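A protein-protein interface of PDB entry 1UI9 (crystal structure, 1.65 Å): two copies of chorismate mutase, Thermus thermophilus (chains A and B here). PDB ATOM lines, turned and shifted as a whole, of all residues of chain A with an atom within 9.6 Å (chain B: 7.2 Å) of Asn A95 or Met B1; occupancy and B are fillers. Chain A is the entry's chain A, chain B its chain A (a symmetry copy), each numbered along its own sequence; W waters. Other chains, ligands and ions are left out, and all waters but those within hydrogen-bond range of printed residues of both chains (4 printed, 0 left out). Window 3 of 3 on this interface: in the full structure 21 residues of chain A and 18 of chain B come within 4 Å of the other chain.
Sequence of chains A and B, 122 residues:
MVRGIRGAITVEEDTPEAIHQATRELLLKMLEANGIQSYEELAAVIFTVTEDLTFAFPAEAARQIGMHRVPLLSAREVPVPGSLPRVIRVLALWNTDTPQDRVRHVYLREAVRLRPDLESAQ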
ATOM      1  N   MET A   1      36.366 -12.747 -19.866  1.00  0.00           N
ATOM      2  CA  MET A   1      35.797 -12.028 -21.042  1.00  0.00           C
ATOM      3  C   MET A   1      34.307 -11.772 -20.843  1.00  0.00           C
ATOM      4  O   MET A   1      33.583 -12.624 -20.319  1.00  0.00           O
ATOM      5  CB  MET A   1      36.013 -12.849 -22.310  1.00  0.00           C
ATOM      6  CG  MET A   1      35.626 -12.131 -23.585  1.00  0.00           C
ATOM      7  SD  MET A   1      36.091 -13.090 -25.030  1.00  0.00           S
ATOM      8  CE  MET A   1      34.484 -13.474 -25.734  1.00  0.00           C
ATOM      9  N   VAL A   2      33.850 -10.601 -21.275  1.00  0.00           N
ATOM     10  CA  VAL A   2      32.451 -10.232 -21.125  1.00  0.00           C
ATOM     11  C   VAL A   2      31.800  -9.821 -22.436  1.00  0.00           C
ATOM     12  O   VAL A   2      32.409  -9.138 -23.264  1.00  0.00           O
ATOM     13  CB  VAL A   2      32.298  -9.068 -20.118  1.00  0.00           C
ATOM     14  CG1 VAL A   2      30.844  -8.627 -20.035  1.00  0.00           C
ATOM     15  CG2 VAL A   2      32.805  -9.504 -18.753  1.00  0.00           C
ATOM     16  N   ARG A   3      30.554 -10.251 -22.612  1.00  0.00           N
ATOM     17  CA  ARG A   3      29.769  -9.929 -23.793  1.00  0.00           C
ATOM     18  C   ARG A   3      28.445  -9.360 -23.325  1.00  0.00           C
ATOM     19  O   ARG A   3      27.782  -9.945 -22.471  1.00  0.00           O
ATOM     20  CB  ARG A   3      29.476 -11.182 -24.625  1.00  0.00           C
ATOM     21  CG  ARG A   3      30.675 -11.772 -25.322  1.00  0.00           C
ATOM     22  CD  ARG A   3      31.261 -10.777 -26.297  1.00  0.00           C
ATOM     23  NE  ARG A   3      32.373 -11.353 -27.043  1.00  0.00           N
ATOM     24  CZ  ARG A   3      33.213 -10.641 -27.787  1.00  0.00           C
ATOM     25  NH1 ARG A   3      33.062  -9.327 -27.881  1.00  0.00           N
ATOM     26  NH2 ARG A   3      34.202 -11.243 -28.436  1.00  0.00           N
ATOM     27  N   GLY A   4      28.062  -8.220 -23.880  1.00  0.00           N
ATOM     28  CA  GLY A   4      26.788  -7.638 -23.514  1.00  0.00           C
ATOM     29  C   GLY A   4      25.692  -8.259 -24.362  1.00  0.00           C
ATOM     30  O   GLY A   4      25.916  -8.627 -25.520  1.00  0.00           O
ATOM     31  N   ILE A   5      24.508  -8.406 -23.783  1.00  0.00           N
ATOM     32  CA  ILE A   5      23.370  -8.945 -24.512  1.00  0.00           C
ATOM     33  C   ILE A   5      22.297  -7.872 -24.445  1.00  0.00           C
ATOM     34  O   ILE A   5      21.988  -7.367 -23.368  1.00  0.00           O
ATOM     35  CB  ILE A   5      22.776 -10.220 -23.865  1.00  0.00           C
ATOM     36  CG1 ILE A   5      23.870 -11.252 -23.572  1.00  0.00           C
ATOM     37  CG2 ILE A   5      21.753 -10.830 -24.817  1.00  0.00           C
ATOM     38  CD1 ILE A   5      23.337 -12.506 -22.901  1.00  0.00           C
ATOM     39  N   ASN A  34      20.433 -17.468 -25.903  1.00  0.00           N
ATOM     40  CA  ASN A  34      21.878 -17.626 -25.769  1.00  0.00           C
ATOM     41  C   ASN A  34      22.297 -18.892 -25.032  1.00  0.00           C
ATOM     42  O   ASN A  34      23.466 -19.056 -24.671  1.00  0.00           O
ATOM     43  CB  ASN A  34      22.456 -16.391 -25.082  1.00  0.00           C
ATOM     44  CG  ASN A  34      22.396 -15.171 -25.968  1.00  0.00           C
ATOM     45  OD1 ASN A  34      23.216 -15.009 -26.871  1.00  0.00           O
ATOM     46  ND2 ASN A  34      21.404 -14.315 -25.738  1.00  0.00           N
ATOM     47  N   ILE A  36      21.896 -19.857 -22.042  1.00  0.00           N
ATOM     48  CA  ILE A  36      22.456 -19.658 -20.713  1.00  0.00           C
ATOM     49  C   ILE A  36      21.828 -20.629 -19.716  1.00  0.00           C
ATOM     50  O   ILE A  36      20.615 -20.644 -19.516  1.00  0.00           O
ATOM     51  CB  ILE A  36      22.272 -18.191 -20.263  1.00  0.00           C
ATOM     52  CG1 ILE A  36      23.059 -17.280 -21.214  1.00  0.00           C
ATOM     53  CG2 ILE A  36      22.765 -18.007 -18.835  1.00  0.00           C
ATOM     54  CD1 ILE A  36      22.936 -15.800 -20.916  1.00  0.00           C
ATOM     55  N   GLN A  37      22.680 -21.440 -19.098  1.00  0.00           N
ATOM     56  CA  GLN A  37      22.260 -22.466 -18.147  1.00  0.00           C
ATOM     57  C   GLN A  37      22.115 -22.000 -16.701  1.00  0.00           C
ATOM     58  O   GLN A  37      21.299 -22.538 -15.952  1.00  0.00           O
ATOM     59  CB  GLN A  37      23.255 -23.629 -18.187  1.00  0.00           C
ATOM     60  CG  GLN A  37      23.480 -24.231 -19.570  1.00  0.00           C
ATOM     61  CD  GLN A  37      22.420 -25.249 -19.951  1.00  0.00           C
ATOM     62  OE1 GLN A  37      21.234 -24.931 -20.026  1.00  0.00           O
ATOM     63  NE2 GLN A  37      22.848 -26.482 -20.195  1.00  0.00           N
ATOM     64  N   SER A  38      22.911 -21.014 -16.301  1.00  0.00           N
ATOM     65  CA  SER A  38      22.865 -20.524 -14.927  1.00  0.00           C
ATOM     66  C   SER A  38      22.987 -19.008 -14.825  1.00  0.00           C
ATOM     67  O   SER A  38      23.665 -18.379 -15.633  1.00  0.00           O
ATOM     68  CB  SER A  38      23.988 -21.172 -14.115  1.00  0.00           C
ATOM     69  OG  SER A  38      24.121 -20.562 -12.842  1.00  0.00           O
ATOM     70  N   TYR A  39      22.336 -18.427 -13.822  1.00  0.00           N
ATOM     71  CA  TYR A  39      22.406 -16.978 -13.627  1.00  0.00           C
ATOM     72  C   TYR A  39      23.805 -16.584 -13.165  1.00  0.00           C
ATOM     73  O   TYR A  39      24.197 -15.427 -13.281  1.00  0.00           O
ATOM     74  CB  TYR A  39      21.390 -16.512 -12.579  1.00  0.00           C
ATOM     75  CG  TYR A  39      19.948 -16.755 -12.952  1.00  0.00           C
ATOM     76  CD1 TYR A  39      19.508 -16.593 -14.264  1.00  0.00           C
ATOM     77  CD2 TYR A  39      19.013 -17.117 -11.983  1.00  0.00           C
ATOM     78  CE1 TYR A  39      18.175 -16.786 -14.604  1.00  0.00           C
ATOM     79  CE2 TYR A  39      17.677 -17.311 -12.312  1.00  0.00           C
ATOM     80  CZ  TYR A  39      17.267 -17.144 -13.624  1.00  0.00           C
ATOM     81  OH  TYR A  39      15.948 -17.329 -13.958  1.00  0.00           O
ATOM     82  N   GLU A  40      24.558 -17.550 -12.644  1.00  0.00           N
ATOM     83  CA  GLU A  40      25.911 -17.283 -12.167  1.00  0.00           C
ATOM     84  C   GLU A  40      26.814 -16.784 -13.292  1.00  0.00           C
ATOM     85  O   GLU A  40      27.899 -16.260 -13.044  1.00  0.00           O
ATOM     86  CB  GLU A  40      26.505 -18.548 -11.534  1.00  0.00           C
ATOM     87  CG  GLU A  40      25.677 -19.074 -10.367  1.00  0.00           C
ATOM     88  CD  GLU A  40      26.277 -20.312  -9.725  1.00  0.00           C
ATOM     89  OE1 GLU A  40      26.526 -21.300 -10.449  1.00  0.00           O
ATOM     90  OE2 GLU A  40      26.493 -20.299  -8.493  1.00  0.00           O
ATOM     91  N   GLU A  41      26.358 -16.950 -14.529  1.00  0.00           N
ATOM     92  CA  GLU A  41      27.116 -16.509 -15.698  1.00  0.00           C
ATOM     93  C   GLU A  41      26.960 -15.009 -15.937  1.00  0.00           C
ATOM     94  O   GLU A  41      27.730 -14.416 -16.691  1.00  0.00           O
ATOM     95  CB  GLU A  41      26.637 -17.246 -16.949  1.00  0.00           C
ATOM     96  CG  GLU A  41      26.912 -18.739 -16.957  1.00  0.00           C
ATOM     97  CD  GLU A  41      26.352 -19.411 -18.194  1.00  0.00           C
ATOM     98  OE1 GLU A  41      26.649 -18.942 -19.312  1.00  0.00           O
ATOM     99  OE2 GLU A  41      25.616 -20.412 -18.050  1.00  0.00           O
ATOM    100  N   LEU A  42      25.962 -14.401 -15.302  1.00  0.00           N
ATOM    101  CA  LEU A  42      25.705 -12.973 -15.479  1.00  0.00           C
ATOM    102  C   LEU A  42      26.436 -12.080 -14.488  1.00  0.00           C
ATOM    103  O   LEU A  42      26.258 -12.200 -13.278  1.00  0.00           O
ATOM    104  CB  LEU A  42      24.201 -12.694 -15.385  1.00  0.00           C
ATOM    105  CG  LEU A  42      23.314 -13.455 -16.373  1.00  0.00           C
ATOM    106  CD1 LEU A  42      21.850 -13.148 -16.085  1.00  0.00           C
ATOM    107  CD2 LEU A  42      23.679 -13.065 -17.800  1.00  0.00           C
ATOM    108  N   ALA A  43      27.253 -11.170 -15.010  1.00  0.00           N
ATOM    109  CA  ALA A  43      27.996 -10.245 -14.165  1.00  0.00           C
ATOM    110  C   ALA A  43      27.029  -9.246 -13.544  1.00  0.00           C
ATOM    111  O   ALA A  43      27.132  -8.911 -12.364  1.00  0.00           O
ATOM    112  CB  ALA A  43      29.042  -9.506 -14.993  1.00  0.00           C
ATOM    113  N   ALA A  44      26.090  -8.776 -14.355  1.00  0.00           N
ATOM    114  CA  ALA A  44      25.096  -7.807 -13.912  1.00  0.00           C
ATOM    115  C   ALA A  44      24.097  -7.585 -15.035  1.00  0.00           C
ATOM    116  O   ALA A  44      24.329  -7.993 -16.169  1.00  0.00           O
ATOM    117  CB  ALA A  44      25.777  -6.488 -13.558  1.00  0.00           C
ATOM    118  N   VAL A  70      21.776 -11.738  -8.845  1.00  0.00           N
ATOM    119  CA  VAL A  70      22.301 -11.012 -10.001  1.00  0.00           C
ATOM    120  C   VAL A  70      22.149  -9.516  -9.740  1.00  0.00           C
ATOM    121  O   VAL A  70      21.041  -9.032  -9.522  1.00  0.00           O
ATOM    122  CB  VAL A  70      21.524 -11.361 -11.289  1.00  0.00           C
ATOM    123  CG1 VAL A  70      22.161 -10.667 -12.489  1.00  0.00           C
ATOM    124  CG2 VAL A  70      21.507 -12.867 -11.492  1.00  0.00           C
ATOM    125  N   PRO A  71      23.262  -8.765  -9.740  1.00  0.00           N
ATOM    126  CA  PRO A  71      23.153  -7.323  -9.493  1.00  0.00           C
ATOM    127  C   PRO A  71      22.391  -6.620 -10.615  1.00  0.00           C
ATOM    128  O   PRO A  71      22.689  -6.797 -11.799  1.00  0.00           O
ATOM    129  CB  PRO A  71      24.612  -6.877  -9.373  1.00  0.00           C
ATOM    130  CG  PRO A  71      25.351  -7.868 -10.195  1.00  0.00           C
ATOM    131  CD  PRO A  71      24.668  -9.177  -9.884  1.00  0.00           C
ATOM    132  N   ALA A  92      22.437  -7.129 -20.532  1.00  0.00           N
ATOM    133  CA  ALA A  92      22.973  -8.129 -19.627  1.00  0.00           C
ATOM    134  C   ALA A  92      24.461  -8.303 -19.910  1.00  0.00           C
ATOM    135  O   ALA A  92      24.854  -8.495 -21.059  1.00  0.00           O
ATOM    136  CB  ALA A  92      22.237  -9.452 -19.828  1.00  0.00           C
ATOM    137  N   LEU A  93      25.286  -8.224 -18.869  1.00  0.00           N
ATOM    138  CA  LEU A  93      26.728  -8.396 -19.025  1.00  0.00           C
ATOM    139  C   LEU A  93      27.006  -9.860 -18.723  1.00  0.00           C
ATOM    140  O   LEU A  93      26.880 -10.321 -17.585  1.00  0.00           O
ATOM    141  CB  LEU A  93      27.483  -7.464 -18.074  1.00  0.00           C
ATOM    142  CG  LEU A  93      27.254  -5.981 -18.389  1.00  0.00           C
ATOM    143  CD1 LEU A  93      27.962  -5.113 -17.363  1.00  0.00           C
ATOM    144  CD2 LEU A  93      27.757  -5.663 -19.798  1.00  0.00           C
ATOM    145  N   TRP A  94      27.384 -10.578 -19.774  1.00  0.00           N
ATOM    146  CA  TRP A  94      27.606 -12.014 -19.723  1.00  0.00           C
ATOM    147  C   TRP A  94      29.067 -12.435 -19.771  1.00  0.00           C
ATOM    148  O   TRP A  94      29.804 -12.052 -20.680  1.00  0.00           O
ATOM    149  CB  TRP A  94      26.813 -12.628 -20.887  1.00  0.00           C
ATOM    150  CG  TRP A  94      26.846 -14.122 -21.064  1.00  0.00           C
ATOM    151  CD1 TRP A  94      26.980 -15.074 -20.096  1.00  0.00           C
ATOM    152  CD2 TRP A  94      26.630 -14.826 -22.294  1.00  0.00           C
ATOM    153  NE1 TRP A  94      26.858 -16.332 -20.650  1.00  0.00           N
ATOM    154  CE2 TRP A  94      26.643 -16.206 -21.997  1.00  0.00           C
ATOM    155  CE3 TRP A  94      26.424 -14.421 -23.620  1.00  0.00           C
ATOM    156  CZ2 TRP A  94      26.457 -17.188 -22.983  1.00  0.00           C
ATOM    157  CZ3 TRP A  94      26.239 -15.396 -24.600  1.00  0.00           C
ATOM    158  CH2 TRP A  94      26.257 -16.763 -24.272  1.00  0.00           C
ATOM    159  N   ASN A  95      29.475 -13.205 -18.764  1.00  0.00           N
ATOM    160  CA  ASN A  95      30.832 -13.738 -18.687  1.00  0.00           C
ATOM    161  C   ASN A  95      30.807 -14.954 -19.602  1.00  0.00           C
ATOM    162  O   ASN A  95      30.225 -15.982 -19.263  1.00  0.00           O
ATOM    163  CB  ASN A  95      31.164 -14.176 -17.259  1.00  0.00           C
ATOM    164  CG  ASN A  95      31.338 -13.007 -16.317  1.00  0.00           C
ATOM    165  OD1 ASN A  95      32.180 -12.139 -16.541  1.00  0.00           O
ATOM    166  ND2 ASN A  95      30.545 -12.978 -15.254  1.00  0.00           N
ATOM    167  N   THR A  96      31.436 -14.828 -20.763  1.00  0.00           N
ATOM    168  CA  THR A  96      31.441 -15.903 -21.738  1.00  0.00           C
ATOM    169  C   THR A  96      32.536 -15.654 -22.763  1.00  0.00           C
ATOM    170  O   THR A  96      33.028 -14.536 -22.891  1.00  0.00           O
ATOM    171  CB  THR A  96      30.081 -15.956 -22.470  1.00  0.00           C
ATOM    172  OG1 THR A  96      30.057 -17.060 -23.381  1.00  0.00           O
ATOM    173  CG2 THR A  96      29.850 -14.667 -23.251  1.00  0.00           C
ATOM    174  N   ASP A  97      32.916 -16.700 -23.489  1.00  0.00           N
ATOM    175  CA  ASP A  97      33.932 -16.570 -24.523  1.00  0.00           C
ATOM    176  C   ASP A  97      33.247 -16.598 -25.886  1.00  0.00           C
ATOM    177  O   ASP A  97      33.903 -16.677 -26.928  1.00  0.00           O
ATOM    178  CB  ASP A  97      34.965 -17.696 -24.410  1.00  0.00           C
ATOM    179  CG  ASP A  97      34.337 -19.042 -24.115  1.00  0.00           C
ATOM    180  OD1 ASP A  97      33.453 -19.475 -24.886  1.00  0.00           O
ATOM    181  OD2 ASP A  97      34.732 -19.669 -23.109  1.00  0.00           O
ATOM    182  N   THR A  98      31.919 -16.526 -25.861  1.00  0.00           N
ATOM    183  CA  THR A  98      31.118 -16.529 -27.078  1.00  0.00           C
ATOM    184  C   THR A  98      31.516 -15.361 -27.980  1.00  0.00           C
ATOM    185  O   THR A  98      31.605 -14.219 -27.525  1.00  0.00           O
ATOM    186  CB  THR A  98      29.610 -16.398 -26.750  1.00  0.00           C
ATOM    187  OG1 THR A  98      29.182 -17.532 -25.989  1.00  0.00           O
ATOM    188  CG2 THR A  98      28.790 -16.304 -28.026  1.00  0.00           C
ATOM    189  N   VAL A 103      26.470 -13.783 -30.262  1.00  0.00           N
ATOM    190  CA  VAL A 103      25.569 -13.411 -29.178  1.00  0.00           C
ATOM    191  C   VAL A 103      24.211 -13.092 -29.796  1.00  0.00           C
ATOM    192  O   VAL A 103      24.134 -12.397 -30.805  1.00  0.00           O
ATOM    193  CB  VAL A 103      26.084 -12.161 -28.422  1.00  0.00           C
ATOM    194  CG1 VAL A 103      25.056 -11.711 -27.395  1.00  0.00           C
ATOM    195  CG2 VAL A 103      27.405 -12.475 -27.738  1.00  0.00           C
ATOM    196  N   MET B   1      36.936 -12.475 -15.691  1.00  0.00           N
ATOM    197  CA  MET B   1      35.570 -12.629 -15.115  1.00  0.00           C
ATOM    198  C   MET B   1      35.168 -11.373 -14.348  1.00  0.00           C
ATOM    199  O   MET B   1      35.990 -10.766 -13.654  1.00  0.00           O
ATOM    200  CB  MET B   1      35.529 -13.837 -14.183  1.00  0.00           C
ATOM    201  CG  MET B   1      34.144 -14.184 -13.680  1.00  0.00           C
ATOM    202  SD  MET B   1      34.163 -15.721 -12.754  1.00  0.00           S
ATOM    203  CE  MET B   1      33.719 -15.151 -11.110  1.00  0.00           C
ATOM    204  N   VAL B   2      33.898 -10.997 -14.464  1.00  0.00           N
ATOM    205  CA  VAL B   2      33.399  -9.805 -13.794  1.00  0.00           C
ATOM    206  C   VAL B   2      32.180 -10.077 -12.928  1.00  0.00           C
ATOM    207  O   VAL B   2      31.292 -10.848 -13.301  1.00  0.00           O
ATOM    208  CB  VAL B   2      33.032  -8.713 -14.826  1.00  0.00           C
ATOM    209  CG1 VAL B   2      32.425  -7.506 -14.127  1.00  0.00           C
ATOM    210  CG2 VAL B   2      34.271  -8.312 -15.609  1.00  0.00           C
ATOM    211  N   ARG B   3      32.154  -9.433 -11.765  1.00  0.00           N
ATOM    212  CA  ARG B   3      31.051  -9.550 -10.824  1.00  0.00           C
ATOM    213  C   ARG B   3      30.594  -8.149 -10.473  1.00  0.00           C
ATOM    214  O   ARG B   3      31.408  -7.295 -10.131  1.00  0.00           O
ATOM    215  CB  ARG B   3      31.495 -10.239  -9.530  1.00  0.00           C
ATOM    216  CG  ARG B   3      31.811 -11.706  -9.671  1.00  0.00           C
ATOM    217  CD  ARG B   3      30.587 -12.468 -10.125  1.00  0.00           C
ATOM    218  NE  ARG B   3      30.845 -13.901 -10.192  1.00  0.00           N
ATOM    219  CZ  ARG B   3      30.030 -14.773 -10.777  1.00  0.00           C
ATOM    220  NH1 ARG B   3      28.909 -14.353 -11.346  1.00  0.00           N
ATOM    221  NH2 ARG B   3      30.339 -16.064 -10.795  1.00  0.00           N
ATOM    222  N   GLY B   4      29.294  -7.913 -10.561  1.00  0.00           N
ATOM    223  CA  GLY B   4      28.777  -6.609 -10.199  1.00  0.00           C
ATOM    224  C   GLY B   4      28.544  -6.561  -8.700  1.00  0.00           C
ATOM    225  O   GLY B   4      28.212  -7.573  -8.075  1.00  0.00           O
ATOM    226  N   GLU B  41      41.219  -3.146  -9.293  1.00  0.00           N
ATOM    227  CA  GLU B  41      40.356  -4.312  -9.465  1.00  0.00           C
ATOM    228  C   GLU B  41      39.002  -3.929 -10.059  1.00  0.00           C
ATOM    229  O   GLU B  41      38.262  -4.792 -10.528  1.00  0.00           O
ATOM    230  CB  GLU B  41      40.113  -4.994  -8.118  1.00  0.00           C
ATOM    231  CG  GLU B  41      41.342  -5.620  -7.486  1.00  0.00           C
ATOM    232  CD  GLU B  41      41.038  -6.216  -6.126  1.00  0.00           C
ATOM    233  OE1 GLU B  41      40.085  -7.017  -6.028  1.00  0.00           O
ATOM    234  OE2 GLU B  41      41.755  -5.889  -5.155  1.00  0.00           O
ATOM    235  N   TRP B  94      33.382  -5.448 -10.856  1.00  0.00           N
ATOM    236  CA  TRP B  94      34.590  -5.981 -10.249  1.00  0.00           C
ATOM    237  C   TRP B  94      35.203  -7.165 -10.981  1.00  0.00           C
ATOM    238  O   TRP B  94      34.531  -8.165 -11.236  1.00  0.00           O
ATOM    239  CB  TRP B  94      34.233  -6.350  -8.800  1.00  0.00           C
ATOM    240  CG  TRP B  94      35.315  -6.914  -7.919  1.00  0.00           C
ATOM    241  CD1 TRP B  94      36.654  -6.654  -7.971  1.00  0.00           C
ATOM    242  CD2 TRP B  94      35.114  -7.759  -6.778  1.00  0.00           C
ATOM    243  NE1 TRP B  94      37.299  -7.285  -6.927  1.00  0.00           N
ATOM    244  CE2 TRP B  94      36.375  -7.969  -6.182  1.00  0.00           C
ATOM    245  CE3 TRP B  94      33.984  -8.356  -6.202  1.00  0.00           C
ATOM    246  CZ2 TRP B  94      36.540  -8.756  -5.031  1.00  0.00           C
ATOM    247  CZ3 TRP B  94      34.146  -9.138  -5.058  1.00  0.00           C
ATOM    248  CH2 TRP B  94      35.418  -9.328  -4.488  1.00  0.00           C
ATOM    249  N   ASN B  95      36.478  -7.022 -11.337  1.00  0.00           N
ATOM    250  CA  ASN B  95      37.229  -8.084 -12.000  1.00  0.00           C
ATOM    251  C   ASN B  95      37.654  -9.005 -10.866  1.00  0.00           C
ATOM    252  O   ASN B  95      38.536  -8.667 -10.081  1.00  0.00           O
ATOM    253  CB  ASN B  95      38.470  -7.519 -12.695  1.00  0.00           C
ATOM    254  CG  ASN B  95      38.130  -6.698 -13.918  1.00  0.00           C
ATOM    255  OD1 ASN B  95      37.495  -7.191 -14.849  1.00  0.00           O
ATOM    256  ND2 ASN B  95      38.555  -5.441 -13.927  1.00  0.00           N
ATOM    257  N   THR B  96      37.016 -10.164 -10.782  1.00  0.00           N
ATOM    258  CA  THR B  96      37.300 -11.107  -9.715  1.00  0.00           C
ATOM    259  C   THR B  96      36.743 -12.473 -10.081  1.00  0.00           C
ATOM    260  O   THR B  96      35.892 -12.585 -10.960  1.00  0.00           O
ATOM    261  CB  THR B  96      36.632 -10.634  -8.405  1.00  0.00           C
ATOM    262  OG1 THR B  96      36.969 -11.522  -7.334  1.00  0.00           O
ATOM    263  CG2 THR B  96      35.116 -10.609  -8.564  1.00  0.00           C
ATOM    264  N   ASP B  97      37.228 -13.509  -9.407  1.00  0.00           N
ATOM    265  CA  ASP B  97      36.742 -14.860  -9.650  1.00  0.00           C
ATOM    266  C   ASP B  97      35.832 -15.266  -8.496  1.00  0.00           C
ATOM    267  O   ASP B  97      35.430 -16.426  -8.378  1.00  0.00           O
ATOM    268  CB  ASP B  97      37.913 -15.839  -9.789  1.00  0.00           C
ATOM    269  CG  ASP B  97      39.011 -15.587  -8.777  1.00  0.00           C
ATOM    270  OD1 ASP B  97      38.721 -15.586  -7.562  1.00  0.00           O
ATOM    271  OD2 ASP B  97      40.171 -15.395  -9.201  1.00  0.00           O
ATOM    272  N   THR B  98      35.509 -14.291  -7.650  1.00  0.00           N
ATOM    273  CA  THR B  98      34.638 -14.513  -6.503  1.00  0.00           C
ATOM    274  C   THR B  98      33.280 -15.046  -6.961  1.00  0.00           C
ATOM    275  O   THR B  98      32.662 -14.488  -7.870  1.00  0.00           O
ATOM    276  CB  THR B  98      34.406 -13.198  -5.720  1.00  0.00           C
ATOM    277  OG1 THR B  98      35.649 -12.726  -5.190  1.00  0.00           O
ATOM    278  CG2 THR B  98      33.421 -13.418  -4.583  1.00  0.00           C
ATOM    279  N   PRO B  99      32.804 -16.143  -6.346  1.00  0.00           N
ATOM    280  CA  PRO B  99      31.509 -16.721  -6.712  1.00  0.00           C
ATOM    281  C   PRO B  99      30.405 -15.680  -6.549  1.00  0.00           C
ATOM    282  O   PRO B  99      30.476 -14.833  -5.664  1.00  0.00           O
ATOM    283  CB  PRO B  99      31.355 -17.873  -5.725  1.00  0.00           C
ATOM    284  CG  PRO B  99      32.768 -18.312  -5.519  1.00  0.00           C
ATOM    285  CD  PRO B  99      33.500 -17.000  -5.370  1.00  0.00           C
ATOM    286  N   GLN B 100      29.390 -15.752  -7.401  1.00  0.00           N
ATOM    287  CA  GLN B 100      28.280 -14.806  -7.356  1.00  0.00           C
ATOM    288  C   GLN B 100      27.635 -14.738  -5.972  1.00  0.00           C
ATOM    289  O   GLN B 100      27.296 -13.655  -5.489  1.00  0.00           O
ATOM    290  CB  GLN B 100      27.230 -15.195  -8.402  1.00  0.00           C
ATOM    291  CG  GLN B 100      26.122 -14.177  -8.593  1.00  0.00           C
ATOM    292  CD  GLN B 100      25.164 -14.576  -9.695  1.00  0.00           C
ATOM    293  OE1 GLN B 100      24.423 -15.554  -9.569  1.00  0.00           O
ATOM    294  NE2 GLN B 100      25.180 -13.827 -10.790  1.00  0.00           N
HETATM  295  O   HOH W   1      27.418 -11.777 -10.777  1.00  0.00           O
HETATM  296  O   HOH W   2      30.558 -18.359 -12.581  1.00  0.00           O
HETATM  297  O   HOH W   3      28.835 -18.025  -9.052  1.00  0.00           O
HETATM  298  O   HOH W   4      27.605 -18.545  -6.814  1.00  0.00           O
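Printed residues of chain B that touch a printed residue of chain A: Met B1, Val B2, Arg B3, Gly B4 and Gln B100.
Hydrophobic or aromatic side chains of chain A within 4 Å of the printed part of chain B: Val A2, Ala A43, Val A70 and Pro A71.
Among the printed residues, no Asp or Glu carboxylate lies within 4 Å of a Lys or Arg side-chain nitrogen of the other chain.
OD1 of Asn A95 sits at hydrogen-bond distance from N of Val B2, at 2.9 Å.
O of Glu A40 sits at hydrogen-bond distance from NH1 of Arg B3 (2.7 Å).
The backbone carbonyl oxygen (O) of Leu A42 lies within hydrogen-bond range of the side-chain amide nitrogen (NE2) of Gln B100 (3.2 Å).
N of Gly B4 is in hydrogen-bond range of O of Ala A43 (3.0 Å).
The side-chain amide nitrogen (NE2) of Gln B100 sits at hydrogen-bond distance from the backbone carbonyl oxygen (O) of Tyr A39 (3.1 Å).
Val B2 touches Val A2 (CG2 to CG2, 3.7 Å).
Gln B100 touches Glu A40 (OE1 to CA, 3.5 Å).
Arg B3 touches Leu A42 (NH1 to O, 3.9 Å).
CB of Ala A43 touches O of Val B2 (3.1 Å).
Val A70 touches Gln B100 (CG2 to NE2, 3.9 Å).
Pro A71 touches Gly B4 (CG to O, 3.6 Å).
OD1 of Asn A95 touches CA of Met B1, 3.7 Å away.
Water W4 bridges the side-chain carboxylate (OE2) of Glu A40 (2.7 Å) and the backbone NH (N) of Gln B100 (3.4 Å).
Water W1 lies within hydrogen-bond range of the backbone carbonyl oxygen (O) of Leu A42, the guanidinium group (NH1) of Arg B3, the side-chain amide nitrogen (NE2) of Gln B100 and the backbone carbonyl oxygen (O) of Ala A43.
Water W3 lies within hydrogen-bond range of the backbone NH of Gln B100 (2.9 Å), the guanidinium group of Arg B3 (3.0 Å) and the side-chain carboxylate of Glu A40 (3.3 Å).
Water W2 bridges the guanidinium group of Arg B3 (2.9 Å) and the backbone carbonyl oxygen of Glu A40 (3.4 Å).
Of chain B, only Met B1 (3.7 Å) and Val B2 (2.9 Å) come within 4 Å of Asn A95.
Of chain A, only Asn A95 comes within 4 Å of Met B1.
Of the printed residues of chain A, Gln B100 touches Tyr A39, Glu A40, Leu A42 and Val A70.
Printed residues of chain A within 4 Å of Gly B4: Ala A43 (3.0 Å) and Pro A71 (3.6 Å).
Of the printed residues of chain B, Ala A43 touches Val B2 (3.1 Å) and Gly B4 (3.0 Å).
Of the printed residues of chain B, Leu A42 touches Arg B3 (3.9 Å) and Gln B100 (3.2 Å).
Of the printed residues of chain B, Glu A40 touches Arg B3 (2.7 Å) and Gln B100 (3.5 Å).
Asn A34 touches none of the printed residues of chain B.
Trp A94 touches none of the printed residues of chain B.
The nearest residue of chain A that does not touch Met B1 is Met A1 (4.2 Å).
The nearest printed residue of chain B that does not touch Tyr A39 is Arg B3 (5.2 Å).
The backbone carbonyl oxygen (O) of Glu A41 sits at hydrogen-bond distance from the backbone NH (N) of Asn A95 (3.0 Å).
The guanidinium group (NE) of Arg B3 is in hydrogen-bond range of the backbone carbonyl oxygen (O) of Thr B98, at 3.0 Å.
The backbone NH (N) of Arg B3 sits at hydrogen-bond distance from the backbone carbonyl oxygen (O) of Trp B94 (2.7 Å).
O of Met B1 is in hydrogen-bond range of N of Thr B96 (3.1 Å).
N of Ala A43 lies within hydrogen-bond range of O of Leu A93 (2.7 Å).
The backbone NH (N) of Glu A40 is in hydrogen-bond range of the side-chain hydroxyl (OG) of Ser A38 (3.0 Å).
Val A2 touches its own counterpart, Val B2.
Asn A95 touches Met B1, but with the chains exchanged Met A1 does not touch Asn B95 (7.6 Å).
Asn A95 touches Val B2, but with the chains exchanged Val A2 does not touch Asn B95 (6.5 Å).
Positions printed for both chains: 1, 2, 3, 4, 41, 94, 95, 96, 97 and 98.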
